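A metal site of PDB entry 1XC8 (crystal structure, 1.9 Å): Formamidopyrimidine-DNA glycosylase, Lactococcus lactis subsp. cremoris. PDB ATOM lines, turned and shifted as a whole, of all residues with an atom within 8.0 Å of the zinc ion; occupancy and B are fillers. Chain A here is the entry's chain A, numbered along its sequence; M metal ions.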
ATOM      1  N   TRP A 179      26.582  21.611 -11.884  1.00  0.00           N
ATOM      2  CA  TRP A 179      25.297  21.677 -12.588  1.00  0.00           C
ATOM      3  C   TRP A 179      25.133  20.439 -13.489  1.00  0.00           C
ATOM      4  O   TRP A 179      24.027  19.824 -13.553  1.00  0.00           O
ATOM      5  CB  TRP A 179      25.184  22.953 -13.429  1.00  0.00           C
ATOM      6  CG  TRP A 179      23.902  23.041 -14.274  1.00  0.00           C
ATOM      7  CD1 TRP A 179      22.688  23.631 -13.897  1.00  0.00           C
ATOM      8  CD2 TRP A 179      23.681  22.529 -15.595  1.00  0.00           C
ATOM      9  NE1 TRP A 179      21.765  23.523 -14.922  1.00  0.00           N
ATOM     10  CE2 TRP A 179      22.336  22.832 -15.956  1.00  0.00           C
ATOM     11  CE3 TRP A 179      24.476  21.808 -16.511  1.00  0.00           C
ATOM     12  CZ2 TRP A 179      21.794  22.480 -17.183  1.00  0.00           C
ATOM     13  CZ3 TRP A 179      23.922  21.454 -17.708  1.00  0.00           C
ATOM     14  CH2 TRP A 179      22.576  21.794 -18.047  1.00  0.00           C
ATOM     15  N   LYS A 182      24.342  17.485 -11.332  1.00  0.00           N
ATOM     16  CA  LYS A 182      23.147  17.694 -10.499  1.00  0.00           C
ATOM     17  C   LYS A 182      23.393  17.633  -8.990  1.00  0.00           C
ATOM     18  O   LYS A 182      22.635  17.003  -8.241  1.00  0.00           O
ATOM     19  CB  LYS A 182      22.033  16.682 -10.897  1.00  0.00           C
ATOM     20  CG  LYS A 182      21.612  16.850 -12.391  1.00  0.00           C
ATOM     21  CD  LYS A 182      20.468  15.868 -12.800  1.00  0.00           C
ATOM     22  CE  LYS A 182      19.914  16.237 -14.164  1.00  0.00           C
ATOM     23  NZ  LYS A 182      18.589  15.533 -14.545  1.00  0.00           N
ATOM     24  N   VAL A 237      25.683  27.703 -16.574  1.00  0.00           N
ATOM     25  CA  VAL A 237      25.363  28.437 -15.342  1.00  0.00           C
ATOM     26  C   VAL A 237      26.273  29.638 -14.978  1.00  0.00           C
ATOM     27  O   VAL A 237      25.806  30.643 -14.427  1.00  0.00           O
ATOM     28  CB  VAL A 237      25.252  27.499 -14.091  1.00  0.00           C
ATOM     29  CG1 VAL A 237      24.043  26.561 -14.248  1.00  0.00           C
ATOM     30  CG2 VAL A 237      26.555  26.644 -13.884  1.00  0.00           C
ATOM     31  N   LYS A 244      17.369  31.166 -17.726  1.00  0.00           N
ATOM     32  CA  LYS A 244      16.627  29.940 -17.420  1.00  0.00           C
ATOM     33  C   LYS A 244      17.508  28.734 -17.683  1.00  0.00           C
ATOM     34  O   LYS A 244      18.191  28.672 -18.716  1.00  0.00           O
ATOM     35  CB  LYS A 244      15.308  29.843 -18.224  1.00  0.00           C
ATOM     36  CG  LYS A 244      14.399  31.135 -18.249  1.00  0.00           C
ATOM     37  CD  LYS A 244      13.824  31.566 -16.852  1.00  0.00           C
ATOM     38  CE  LYS A 244      12.946  32.873 -16.925  1.00  0.00           C
ATOM     39  NZ  LYS A 244      12.453  33.392 -15.531  1.00  0.00           N
ATOM     40  N   CYS A 245      17.530  27.798 -16.727  1.00  0.00           N
ATOM     41  CA  CYS A 245      18.194  26.495 -16.896  1.00  0.00           C
ATOM     42  C   CYS A 245      17.739  25.820 -18.177  1.00  0.00           C
ATOM     43  O   CYS A 245      16.552  25.713 -18.411  1.00  0.00           O
ATOM     44  CB  CYS A 245      17.889  25.591 -15.706  1.00  0.00           C
ATOM     45  SG  CYS A 245      18.591  23.954 -15.836  1.00  0.00           S
ATOM     46  N   SER A 246      18.689  25.371 -18.986  1.00  0.00           N
ATOM     47  CA  SER A 246      18.410  24.683 -20.243  1.00  0.00           C
ATOM     48  C   SER A 246      17.686  23.318 -20.090  1.00  0.00           C
ATOM     49  O   SER A 246      17.174  22.776 -21.098  1.00  0.00           O
ATOM     50  CB  SER A 246      19.712  24.503 -21.027  1.00  0.00           C
ATOM     51  OG  SER A 246      20.537  23.467 -20.449  1.00  0.00           O
ATOM     52  N   ARG A 247      17.693  22.760 -18.871  1.00  0.00           N
ATOM     53  CA  ARG A 247      17.074  21.451 -18.611  1.00  0.00           C
ATOM     54  C   ARG A 247      15.655  21.574 -18.087  1.00  0.00           C
ATOM     55  O   ARG A 247      14.775  20.852 -18.519  1.00  0.00           O
ATOM     56  CB  ARG A 247      17.893  20.591 -17.603  1.00  0.00           C
ATOM     57  CG  ARG A 247      19.108  19.902 -18.256  1.00  0.00           C
ATOM     58  CD  ARG A 247      19.844  18.900 -17.285  1.00  0.00           C
ATOM     59  NE  ARG A 247      20.173  19.601 -16.045  1.00  0.00           N
ATOM     60  CZ  ARG A 247      21.285  19.437 -15.352  1.00  0.00           C
ATOM     61  NH1 ARG A 247      22.204  18.541 -15.728  1.00  0.00           N
ATOM     62  NH2 ARG A 247      21.468  20.157 -14.259  1.00  0.00           N
ATOM     63  N   CYS A 248      15.434  22.482 -17.173  1.00  0.00           N
ATOM     64  CA  CYS A 248      14.162  22.514 -16.466  1.00  0.00           C
ATOM     65  C   CYS A 248      13.384  23.843 -16.626  1.00  0.00           C
ATOM     66  O   CYS A 248      12.190  23.871 -16.316  1.00  0.00           O
ATOM     67  CB  CYS A 248      14.374  22.184 -14.991  1.00  0.00           C
ATOM     68  SG  CYS A 248      14.986  23.489 -14.029  1.00  0.00           S
ATOM     69  N   GLY A 249      14.065  24.924 -17.050  1.00  0.00           N
ATOM     70  CA  GLY A 249      13.428  26.235 -17.211  1.00  0.00           C
ATOM     71  C   GLY A 249      13.417  27.064 -15.954  1.00  0.00           C
ATOM     72  O   GLY A 249      13.006  28.215 -15.978  1.00  0.00           O
ATOM     73  N   ALA A 250      13.916  26.537 -14.826  1.00  0.00           N
ATOM     74  CA  ALA A 250      14.006  27.394 -13.634  1.00  0.00           C
ATOM     75  C   ALA A 250      15.086  28.465 -13.870  1.00  0.00           C
ATOM     76  O   ALA A 250      15.956  28.246 -14.728  1.00  0.00           O
ATOM     77  CB  ALA A 250      14.351  26.590 -12.408  1.00  0.00           C
ATOM     78  N   GLU A 251      15.028  29.579 -13.118  1.00  0.00           N
ATOM     79  CA  GLU A 251      16.025  30.683 -13.185  1.00  0.00           C
ATOM     80  C   GLU A 251      17.288  30.307 -12.405  1.00  0.00           C
ATOM     81  O   GLU A 251      17.203  29.939 -11.229  1.00  0.00           O
ATOM     82  CB  GLU A 251      15.491  31.994 -12.598  1.00  0.00           C
ATOM     83  CG  GLU A 251      14.784  32.843 -13.588  1.00  0.00           C
ATOM     84  CD  GLU A 251      14.431  34.267 -13.117  1.00  0.00           C
ATOM     85  OE1 GLU A 251      14.998  34.839 -12.140  1.00  0.00           O
ATOM     86  OE2 GLU A 251      13.536  34.811 -13.788  1.00  0.00           O
ATOM     87  N   ILE A 252      18.439  30.443 -13.058  1.00  0.00           N
ATOM     88  CA  ILE A 252      19.721  30.272 -12.357  1.00  0.00           C
ATOM     89  C   ILE A 252      19.863  31.296 -11.263  1.00  0.00           C
ATOM     90  O   ILE A 252      19.614  32.525 -11.456  1.00  0.00           O
ATOM     91  CB  ILE A 252      20.950  30.374 -13.372  1.00  0.00           C
ATOM     92  CG1 ILE A 252      20.799  29.395 -14.529  1.00  0.00           C
ATOM     93  CG2 ILE A 252      22.293  30.229 -12.641  1.00  0.00           C
ATOM     94  CD1 ILE A 252      20.504  27.879 -14.132  1.00  0.00           C
ATOM     95  N   PHE A 264      23.939  28.298  -9.797  1.00  0.00           N
ATOM     96  CA  PHE A 264      23.321  26.956  -9.798  1.00  0.00           C
ATOM     97  C   PHE A 264      21.814  27.003 -10.174  1.00  0.00           C
ATOM     98  O   PHE A 264      21.189  28.056 -10.034  1.00  0.00           O
ATOM     99  CB  PHE A 264      23.537  26.309  -8.416  1.00  0.00           C
ATOM    100  CG  PHE A 264      22.631  26.864  -7.338  1.00  0.00           C
ATOM    101  CD1 PHE A 264      22.824  28.165  -6.829  1.00  0.00           C
ATOM    102  CD2 PHE A 264      21.546  26.113  -6.853  1.00  0.00           C
ATOM    103  CE1 PHE A 264      21.948  28.711  -5.849  1.00  0.00           C
ATOM    104  CE2 PHE A 264      20.704  26.637  -5.873  1.00  0.00           C
ATOM    105  CZ  PHE A 264      20.887  27.928  -5.365  1.00  0.00           C
ATOM    106  N   CYS A 265      21.270  25.869 -10.672  1.00  0.00           N
ATOM    107  CA  CYS A 265      19.826  25.676 -10.821  1.00  0.00           C
ATOM    108  C   CYS A 265      19.280  24.991  -9.531  1.00  0.00           C
ATOM    109  O   CYS A 265      19.727  23.897  -9.157  1.00  0.00           O
ATOM    110  CB  CYS A 265      19.478  24.846 -12.075  1.00  0.00           C
ATOM    111  SG  CYS A 265      17.676  24.210 -12.311  1.00  0.00           S
ATOM    112  N   PRO A 266      18.345  25.675  -8.846  1.00  0.00           N
ATOM    113  CA  PRO A 266      17.767  25.238  -7.568  1.00  0.00           C
ATOM    114  C   PRO A 266      16.840  24.042  -7.737  1.00  0.00           C
ATOM    115  O   PRO A 266      16.569  23.379  -6.720  1.00  0.00           O
ATOM    116  CB  PRO A 266      16.960  26.458  -7.095  1.00  0.00           C
ATOM    117  CG  PRO A 266      17.359  27.585  -7.996  1.00  0.00           C
ATOM    118  CD  PRO A 266      17.744  26.943  -9.296  1.00  0.00           C
ATOM    119  N   VAL A 267      16.401  23.738  -8.956  1.00  0.00           N
ATOM    120  CA  VAL A 267      15.567  22.554  -9.247  1.00  0.00           C
ATOM    121  C   VAL A 267      16.461  21.327  -9.510  1.00  0.00           C
ATOM    122  O   VAL A 267      16.294  20.263  -8.891  1.00  0.00           O
ATOM    123  CB  VAL A 267      14.632  22.791 -10.453  1.00  0.00           C
ATOM    124  CG1 VAL A 267      14.032  21.480 -11.000  1.00  0.00           C
ATOM    125  CG2 VAL A 267      13.496  23.783 -10.041  1.00  0.00           C
ATOM    126  N   CYS A 268      17.436  21.499 -10.398  1.00  0.00           N
ATOM    127  CA  CYS A 268      18.307  20.400 -10.835  1.00  0.00           C
ATOM    128  C   CYS A 268      19.364  20.026  -9.795  1.00  0.00           C
ATOM    129  O   CYS A 268      19.908  18.903  -9.834  1.00  0.00           O
ATOM    130  CB  CYS A 268      19.019  20.805 -12.090  1.00  0.00           C
ATOM    131  SG  CYS A 268      18.075  20.825 -13.584  1.00  0.00           S
ATOM    132  N   GLN A 269      19.696  20.979  -8.914  1.00  0.00           N
ATOM    133  CA  GLN A 269      20.698  20.807  -7.903  1.00  0.00           C
ATOM    134  C   GLN A 269      20.099  20.957  -6.510  1.00  0.00           C
ATOM    135  O   GLN A 269      20.276  21.982  -5.843  1.00  0.00           O
ATOM    136  CB  GLN A 269      21.882  21.807  -8.117  1.00  0.00           C
ATOM    137  CG  GLN A 269      22.614  21.606  -9.482  1.00  0.00           C
ATOM    138  CD  GLN A 269      23.556  22.796  -9.769  1.00  0.00           C
ATOM    139  OE1 GLN A 269      23.214  23.696 -10.548  1.00  0.00           O
ATOM    140  NE2 GLN A 269      24.745  22.806  -9.108  1.00  0.00           N
HETATM  141 ZN    ZN M   1      17.399  23.113 -13.905  1.00  0.00          ZN
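Within 4 Å of the zinc ion: Cys 245, Cys 248, Cys 265 and Cys 268. The nearest printed residue that does not touch the zinc ion is Val 267 (4.4 Å).
The zinc ion is bound by the side-chain sulfur (SG) of Cys 265 (2.0 Å), the side-chain sulfur (SG) of Cys 268 (2.4 Å), the side-chain sulfur (SG) of Cys 245 (2.4 Å) and the side-chain sulfur (SG) of Cys 248 (2.4 Å).
The side-chain sulfur of Cys 265 sits close to the backbone NH of Val 267 (3.6 Å). The side-chain amide oxygen of Gln 269 lies within hydrogen-bond range of the backbone NH of Cys 265, at 2.9 Å. The guanidinium group (NE) of Arg 247 sits close to the side-chain sulfur (SG) of Cys 268, at 3.5 Å. The indole nitrogen (NE1) of Trp 179 sits close to the side-chain sulfur (SG) of Cys 245 (3.3 Å). The side-chain sulfur (SG) of Cys 245 lies close to the backbone NH (N) of Arg 247 (3.4 Å). The backbone carbonyl oxygen (O) of Ala 250 sits at hydrogen-bond distance from the backbone NH (N) of Cys 245, at 2.6 Å. SG of Cys 248 sits close to N of Ala 250, 3.3 Å away.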
